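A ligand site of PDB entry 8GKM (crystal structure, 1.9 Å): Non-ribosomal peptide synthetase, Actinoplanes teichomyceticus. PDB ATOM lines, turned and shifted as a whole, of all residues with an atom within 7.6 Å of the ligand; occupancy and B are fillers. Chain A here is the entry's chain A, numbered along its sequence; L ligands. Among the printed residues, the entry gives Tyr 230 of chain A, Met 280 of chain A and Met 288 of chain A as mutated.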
ATOM      1  N   SER A 147     -21.053  11.582 -15.464  1.00  0.00           N
ATOM      2  CA  SER A 147     -22.339  11.857 -16.114  1.00  0.00           C
ATOM      3  C   SER A 147     -22.111  12.810 -17.278  1.00  0.00           C
ATOM      4  O   SER A 147     -22.693  13.888 -17.369  1.00  0.00           O
ATOM      5  CB  SER A 147     -23.341  12.452 -15.127  1.00  0.00           C
ATOM      6  OG  SER A 147     -22.788  13.558 -14.435  1.00  0.00           O
ATOM      7  N   TRP A 172     -12.503  11.529   8.408  1.00  0.00           N
ATOM      8  CA  TRP A 172     -13.759  10.791   8.421  1.00  0.00           C
ATOM      9  C   TRP A 172     -14.215  10.468   9.837  1.00  0.00           C
ATOM     10  O   TRP A 172     -15.419  10.448  10.115  1.00  0.00           O
ATOM     11  CB  TRP A 172     -13.612   9.497   7.632  1.00  0.00           C
ATOM     12  CG  TRP A 172     -13.501   9.706   6.165  1.00  0.00           C
ATOM     13  CD1 TRP A 172     -12.444   9.382   5.376  1.00  0.00           C
ATOM     14  CD2 TRP A 172     -14.488  10.289   5.305  1.00  0.00           C
ATOM     15  NE1 TRP A 172     -12.709   9.713   4.066  1.00  0.00           N
ATOM     16  CE2 TRP A 172     -13.959  10.281   3.997  1.00  0.00           C
ATOM     17  CE3 TRP A 172     -15.756  10.827   5.520  1.00  0.00           C
ATOM     18  CZ2 TRP A 172     -14.653  10.784   2.914  1.00  0.00           C
ATOM     19  CZ3 TRP A 172     -16.451  11.326   4.428  1.00  0.00           C
ATOM     20  CH2 TRP A 172     -15.906  11.295   3.150  1.00  0.00           C
ATOM     21  N   PHE A 188     -20.747   4.877  -8.412  1.00  0.00           N
ATOM     22  CA  PHE A 188     -20.599   6.269  -7.996  1.00  0.00           C
ATOM     23  C   PHE A 188     -19.574   6.329  -6.872  1.00  0.00           C
ATOM     24  O   PHE A 188     -19.534   5.441  -6.012  1.00  0.00           O
ATOM     25  CB  PHE A 188     -21.921   6.864  -7.508  1.00  0.00           C
ATOM     26  CG  PHE A 188     -22.983   7.002  -8.571  1.00  0.00           C
ATOM     27  CD1 PHE A 188     -22.724   6.674  -9.892  1.00  0.00           C
ATOM     28  CD2 PHE A 188     -24.245   7.467  -8.239  1.00  0.00           C
ATOM     29  CE1 PHE A 188     -23.707   6.805 -10.859  1.00  0.00           C
ATOM     30  CE2 PHE A 188     -25.227   7.605  -9.187  1.00  0.00           C
ATOM     31  CZ  PHE A 188     -24.958   7.275 -10.508  1.00  0.00           C
ATOM     32  N   ASP A 189     -18.742   7.369  -6.842  1.00  0.00           N
ATOM     33  CA  ASP A 189     -17.633   7.318  -5.894  1.00  0.00           C
ATOM     34  C   ASP A 189     -18.036   7.645  -4.455  1.00  0.00           C
ATOM     35  O   ASP A 189     -17.192   7.530  -3.561  1.00  0.00           O
ATOM     36  CB  ASP A 189     -16.470   8.196  -6.370  1.00  0.00           C
ATOM     37  CG  ASP A 189     -16.845   9.644  -6.540  1.00  0.00           C
ATOM     38  OD1 ASP A 189     -17.936  10.051  -6.087  1.00  0.00           O
ATOM     39  OD2 ASP A 189     -16.030  10.385  -7.123  1.00  0.00           O
ATOM     40  N   ALA A 190     -19.308   7.993  -4.193  1.00  0.00           N
ATOM     41  CA  ALA A 190     -19.774   8.012  -2.808  1.00  0.00           C
ATOM     42  C   ALA A 190     -19.665   6.636  -2.163  1.00  0.00           C
ATOM     43  O   ALA A 190     -19.592   6.539  -0.926  1.00  0.00           O
ATOM     44  CB  ALA A 190     -21.221   8.509  -2.737  1.00  0.00           C
ATOM     45  N   SER A 191     -19.671   5.571  -2.971  1.00  0.00           N
ATOM     46  CA  SER A 191     -19.443   4.229  -2.456  1.00  0.00           C
ATOM     47  C   SER A 191     -18.085   4.078  -1.797  1.00  0.00           C
ATOM     48  O   SER A 191     -17.897   3.164  -0.989  1.00  0.00           O
ATOM     49  CB  SER A 191     -19.598   3.223  -3.604  1.00  0.00           C
ATOM     50  OG  SER A 191     -18.617   3.442  -4.599  1.00  0.00           O
ATOM     51  N   PHE A 193     -16.981   6.042   0.436  1.00  0.00           N
ATOM     52  CA  PHE A 193     -17.273   6.248   1.842  1.00  0.00           C
ATOM     53  C   PHE A 193     -18.081   5.078   2.405  1.00  0.00           C
ATOM     54  O   PHE A 193     -17.808   4.610   3.522  1.00  0.00           O
ATOM     55  CB  PHE A 193     -18.031   7.556   2.067  1.00  0.00           C
ATOM     56  CG  PHE A 193     -18.604   7.666   3.444  1.00  0.00           C
ATOM     57  CD1 PHE A 193     -17.794   7.999   4.523  1.00  0.00           C
ATOM     58  CD2 PHE A 193     -19.936   7.376   3.678  1.00  0.00           C
ATOM     59  CE1 PHE A 193     -18.320   8.081   5.800  1.00  0.00           C
ATOM     60  CE2 PHE A 193     -20.471   7.460   4.955  1.00  0.00           C
ATOM     61  CZ  PHE A 193     -19.649   7.805   6.018  1.00  0.00           C
ATOM     62  N   TYR A 230     -24.813   8.309   4.217  1.00  0.00           N
ATOM     63  CA  TYR A 230     -24.710   9.305   3.152  1.00  0.00           C
ATOM     64  C   TYR A 230     -26.013   9.301   2.358  1.00  0.00           C
ATOM     65  O   TYR A 230     -26.580   8.250   2.077  1.00  0.00           O
ATOM     66  CB  TYR A 230     -23.537   8.995   2.210  1.00  0.00           C
ATOM     67  CG  TYR A 230     -23.606   9.755   0.906  1.00  0.00           C
ATOM     68  CD1 TYR A 230     -23.143  11.061   0.807  1.00  0.00           C
ATOM     69  CD2 TYR A 230     -24.165   9.169  -0.226  1.00  0.00           C
ATOM     70  CE1 TYR A 230     -23.203  11.757  -0.385  1.00  0.00           C
ATOM     71  CE2 TYR A 230     -24.235   9.863  -1.427  1.00  0.00           C
ATOM     72  CZ  TYR A 230     -23.755  11.154  -1.500  1.00  0.00           C
ATOM     73  OH  TYR A 230     -23.827  11.843  -2.687  1.00  0.00           O
ATOM     74  N   THR A 255     -23.774  14.368   2.986  1.00  0.00           N
ATOM     75  CA  THR A 255     -24.423  14.650   1.709  1.00  0.00           C
ATOM     76  C   THR A 255     -23.524  15.511   0.845  1.00  0.00           C
ATOM     77  O   THR A 255     -22.528  16.065   1.303  1.00  0.00           O
ATOM     78  CB  THR A 255     -25.789  15.329   1.905  1.00  0.00           C
ATOM     79  OG1 THR A 255     -26.472  15.415   0.646  1.00  0.00           O
ATOM     80  CG2 THR A 255     -25.620  16.734   2.466  1.00  0.00           C
ATOM     81  N   GLY A 256     -23.899  15.617  -0.420  1.00  0.00           N
ATOM     82  CA  GLY A 256     -23.152  16.418  -1.359  1.00  0.00           C
ATOM     83  C   GLY A 256     -23.427  15.930  -2.765  1.00  0.00           C
ATOM     84  O   GLY A 256     -24.188  14.991  -2.993  1.00  0.00           O
ATOM     85  N   GLY A 257     -22.783  16.604  -3.710  1.00  0.00           N
ATOM     86  CA  GLY A 257     -22.957  16.284  -5.116  1.00  0.00           C
ATOM     87  C   GLY A 257     -23.649  17.400  -5.867  1.00  0.00           C
ATOM     88  O   GLY A 257     -23.030  18.109  -6.662  1.00  0.00           O
ATOM     89  N   ASP A 258     -24.943  17.562  -5.614  1.00  0.00           N
ATOM     90  CA  ASP A 258     -25.734  18.641  -6.181  1.00  0.00           C
ATOM     91  C   ASP A 258     -25.964  19.706  -5.109  1.00  0.00           C
ATOM     92  O   ASP A 258     -25.487  19.592  -3.977  1.00  0.00           O
ATOM     93  CB  ASP A 258     -27.052  18.095  -6.730  1.00  0.00           C
ATOM     94  CG  ASP A 258     -27.625  18.939  -7.842  1.00  0.00           C
ATOM     95  OD1 ASP A 258     -27.041  20.005  -8.143  1.00  0.00           O
ATOM     96  OD2 ASP A 258     -28.664  18.545  -8.406  1.00  0.00           O
ATOM     97  N   HIS A 279     -21.352  18.220   4.903  1.00  0.00           N
ATOM     98  CA  HIS A 279     -21.580  18.586   3.511  1.00  0.00           C
ATOM     99  C   HIS A 279     -20.274  18.408   2.755  1.00  0.00           C
ATOM    100  O   HIS A 279     -19.229  18.891   3.196  1.00  0.00           O
ATOM    101  CB  HIS A 279     -22.065  20.044   3.398  1.00  0.00           C
ATOM    102  CG  HIS A 279     -22.333  20.468   1.995  1.00  0.00           C
ATOM    103  ND1 HIS A 279     -21.857  21.656   1.467  1.00  0.00           N
ATOM    104  CD2 HIS A 279     -23.008  19.866   0.985  1.00  0.00           C
ATOM    105  CE1 HIS A 279     -22.242  21.768   0.211  1.00  0.00           C
ATOM    106  NE2 HIS A 279     -22.935  20.691  -0.105  1.00  0.00           N
ATOM    107  N   MET A 280     -20.326  17.702   1.630  1.00  0.00           N
ATOM    108  CA  MET A 280     -19.136  17.329   0.886  1.00  0.00           C
ATOM    109  C   MET A 280     -19.213  17.854  -0.537  1.00  0.00           C
ATOM    110  O   MET A 280     -20.291  17.988  -1.120  1.00  0.00           O
ATOM    111  CB  MET A 280     -18.976  15.800   0.876  1.00  0.00           C
ATOM    112  CG  MET A 280     -18.870  15.201   2.263  1.00  0.00           C
ATOM    113  SD  MET A 280     -18.757  13.404   2.224  1.00  0.00           S
ATOM    114  CE  MET A 280     -20.350  12.971   1.538  1.00  0.00           C
ATOM    115  N   TYR A 281     -18.036  18.171  -1.087  1.00  0.00           N
ATOM    116  CA  TYR A 281     -17.921  18.699  -2.448  1.00  0.00           C
ATOM    117  C   TYR A 281     -16.752  18.031  -3.145  1.00  0.00           C
ATOM    118  O   TYR A 281     -15.663  17.904  -2.566  1.00  0.00           O
ATOM    119  CB  TYR A 281     -17.725  20.231  -2.461  1.00  0.00           C
ATOM    120  CG  TYR A 281     -17.262  20.773  -3.795  1.00  0.00           C
ATOM    121  CD1 TYR A 281     -15.906  20.851  -4.106  1.00  0.00           C
ATOM    122  CD2 TYR A 281     -18.172  21.209  -4.740  1.00  0.00           C
ATOM    123  CE1 TYR A 281     -15.484  21.338  -5.329  1.00  0.00           C
ATOM    124  CE2 TYR A 281     -17.759  21.707  -5.966  1.00  0.00           C
ATOM    125  CZ  TYR A 281     -16.407  21.761  -6.256  1.00  0.00           C
ATOM    126  OH  TYR A 281     -15.965  22.252  -7.460  1.00  0.00           O
ATOM    127  N   GLY A 282     -16.942  17.635  -4.400  1.00  0.00           N
ATOM    128  CA  GLY A 282     -15.821  17.210  -5.194  1.00  0.00           C
ATOM    129  C   GLY A 282     -16.209  16.376  -6.398  1.00  0.00           C
ATOM    130  O   GLY A 282     -17.150  15.581  -6.359  1.00  0.00           O
ATOM    131  N   PRO A 283     -15.450  16.535  -7.474  1.00  0.00           N
ATOM    132  CA  PRO A 283     -15.728  15.755  -8.685  1.00  0.00           C
ATOM    133  C   PRO A 283     -15.107  14.372  -8.622  1.00  0.00           C
ATOM    134  O   PRO A 283     -14.243  14.072  -7.794  1.00  0.00           O
ATOM    135  CB  PRO A 283     -15.101  16.607  -9.788  1.00  0.00           C
ATOM    136  CG  PRO A 283     -13.921  17.241  -9.115  1.00  0.00           C
ATOM    137  CD  PRO A 283     -14.372  17.523  -7.698  1.00  0.00           C
ATOM    138  N   THR A 284     -15.596  13.502  -9.512  1.00  0.00           N
ATOM    139  CA  THR A 284     -15.036  12.166  -9.626  1.00  0.00           C
ATOM    140  C   THR A 284     -13.552  12.221  -9.936  1.00  0.00           C
ATOM    141  O   THR A 284     -12.799  11.320  -9.538  1.00  0.00           O
ATOM    142  CB  THR A 284     -15.759  11.397 -10.738  1.00  0.00           C
ATOM    143  OG1 THR A 284     -17.156  11.319 -10.446  1.00  0.00           O
ATOM    144  CG2 THR A 284     -15.181   9.992 -10.879  1.00  0.00           C
ATOM    145  N   GLU A 285     -13.119  13.265 -10.641  1.00  0.00           N
ATOM    146  CA  GLU A 285     -11.730  13.408 -11.046  1.00  0.00           C
ATOM    147  C   GLU A 285     -10.784  13.595  -9.861  1.00  0.00           C
ATOM    148  O   GLU A 285      -9.568  13.460 -10.032  1.00  0.00           O
ATOM    149  CB  GLU A 285     -11.606  14.588 -12.003  1.00  0.00           C
ATOM    150  CG  GLU A 285     -12.182  14.355 -13.399  1.00  0.00           C
ATOM    151  CD  GLU A 285     -13.673  14.646 -13.523  1.00  0.00           C
ATOM    152  OE1 GLU A 285     -14.372  14.712 -12.488  1.00  0.00           O
ATOM    153  OE2 GLU A 285     -14.144  14.796 -14.670  1.00  0.00           O
ATOM    154  N   THR A 286     -11.287  13.921  -8.675  1.00  0.00           N
ATOM    155  CA  THR A 286     -10.435  14.038  -7.487  1.00  0.00           C
ATOM    156  C   THR A 286     -10.889  13.126  -6.348  1.00  0.00           C
ATOM    157  O   THR A 286     -10.672  13.441  -5.170  1.00  0.00           O
ATOM    158  CB  THR A 286     -10.338  15.490  -7.028  1.00  0.00           C
ATOM    159  OG1 THR A 286     -11.632  16.002  -6.703  1.00  0.00           O
ATOM    160  CG2 THR A 286      -9.699  16.358  -8.117  1.00  0.00           C
ATOM    161  N   THR A 287     -11.509  11.997  -6.680  1.00  0.00           N
ATOM    162  CA  THR A 287     -11.802  10.891  -5.775  1.00  0.00           C
ATOM    163  C   THR A 287     -12.770  11.284  -4.652  1.00  0.00           C
ATOM    164  O   THR A 287     -12.373  11.524  -3.498  1.00  0.00           O
ATOM    165  CB  THR A 287     -10.507  10.320  -5.199  1.00  0.00           C
ATOM    166  OG1 THR A 287      -9.557  10.121  -6.259  1.00  0.00           O
ATOM    167  CG2 THR A 287     -10.788   8.975  -4.543  1.00  0.00           C
ATOM    168  N   MET A 288     -14.037  11.331  -5.026  1.00  0.00           N
ATOM    169  CA  MET A 288     -15.213  11.499  -4.187  1.00  0.00           C
ATOM    170  C   MET A 288     -15.408  12.914  -3.652  1.00  0.00           C
ATOM    171  O   MET A 288     -16.397  13.569  -3.978  1.00  0.00           O
ATOM    172  CB  MET A 288     -15.210  10.539  -2.993  1.00  0.00           C
ATOM    173  CG  MET A 288     -16.581  10.510  -2.311  1.00  0.00           C
ATOM    174  SD  MET A 288     -16.673   9.720  -0.703  1.00  0.00           S
ATOM    175  CE  MET A 288     -18.172  10.473  -0.074  1.00  0.00           C
ATOM    176  N   CYS A 289     -14.535  13.367  -2.755  1.00  0.00           N
ATOM    177  CA  CYS A 289     -14.699  14.720  -2.250  1.00  0.00           C
ATOM    178  C   CYS A 289     -13.339  15.316  -1.930  1.00  0.00           C
ATOM    179  O   CYS A 289     -12.428  14.633  -1.468  1.00  0.00           O
ATOM    180  CB  CYS A 289     -15.606  14.766  -1.011  1.00  0.00           C
ATOM    181  SG  CYS A 289     -15.092  13.779   0.413  1.00  0.00           S
ATOM    182  N   ALA A 290     -13.241  16.619  -2.189  1.00  0.00           N
ATOM    183  CA  ALA A 290     -12.030  17.405  -2.003  1.00  0.00           C
ATOM    184  C   ALA A 290     -12.154  18.440  -0.904  1.00  0.00           C
ATOM    185  O   ALA A 290     -11.148  18.824  -0.323  1.00  0.00           O
ATOM    186  CB  ALA A 290     -11.642  18.104  -3.310  1.00  0.00           C
ATOM    187  N   THR A 291     -13.359  18.935  -0.631  1.00  0.00           N
ATOM    188  CA  THR A 291     -13.595  19.849   0.470  1.00  0.00           C
ATOM    189  C   THR A 291     -14.849  19.395   1.211  1.00  0.00           C
ATOM    190  O   THR A 291     -15.721  18.731   0.650  1.00  0.00           O
ATOM    191  CB  THR A 291     -13.773  21.309   0.023  1.00  0.00           C
ATOM    192  OG1 THR A 291     -15.073  21.508  -0.551  1.00  0.00           O
ATOM    193  CG2 THR A 291     -12.712  21.689  -1.000  1.00  0.00           C
HETATM  194  N1  LIG L   1     -17.889  12.866  -6.303  1.00  0.00           N
HETATM  195  C1  LIG L   1     -19.314  13.138  -6.185  1.00  0.00           C
HETATM  196  C2  LIG L   1     -19.846  13.688  -7.504  1.00  0.00           C
HETATM  197  O1  LIG L   1     -21.087  13.835  -7.682  1.00  0.00           O
HETATM  198  C3  LIG L   1     -19.489  14.172  -5.083  1.00  0.00           C
HETATM  199  C4  LIG L   1     -19.987  13.600  -3.756  1.00  0.00           C
HETATM  200  C5  LIG L   1     -19.515  12.193  -3.424  1.00  0.00           C
HETATM  201  C6  LIG L   1     -19.580  14.543  -2.598  1.00  0.00           C
HETATM  202  O2  LIG L   1     -19.053  13.994  -8.426  1.00  0.00           O
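N of Met 280 sits at hydrogen-bond distance from O of Thr 255.
OD2 of Asp 189 is in hydrogen-bond range of N of Met 288 (3.0 Å).
The side-chain hydroxyl of Thr 286 sits close to the backbone carbonyl oxygen of Pro 283 (3.4 Å).
Residues that only touch the ligand: Thr 284 (3.7 Å), Met 280 (3.7 Å), Pro 283 (3.8 Å) and Gly 257 (3.97 Å).
Hydrophobic or aromatic side chains within 4 Å of the ligand: Met 280 and Met 288.
Seven residues have an atom within 4 Å of the ligand: Asp 189, Gly 257, Met 280, Gly 282, Pro 283, Thr 284 and Met 288.
Along chain A the residues within 4 Å of the ligand span positions 189 to 288.
The nearest printed residue that does not touch the ligand is Gly 256 (4.1 Å).
O of Gly 282 lies within hydrogen-bond range of N1 of the ligand.
O of Met 288 is in hydrogen-bond range of N1 of the ligand (2.9 Å).
OD1 of Asp 189 lies within salt-bridge range of N1 of the ligand (2.8 Å).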
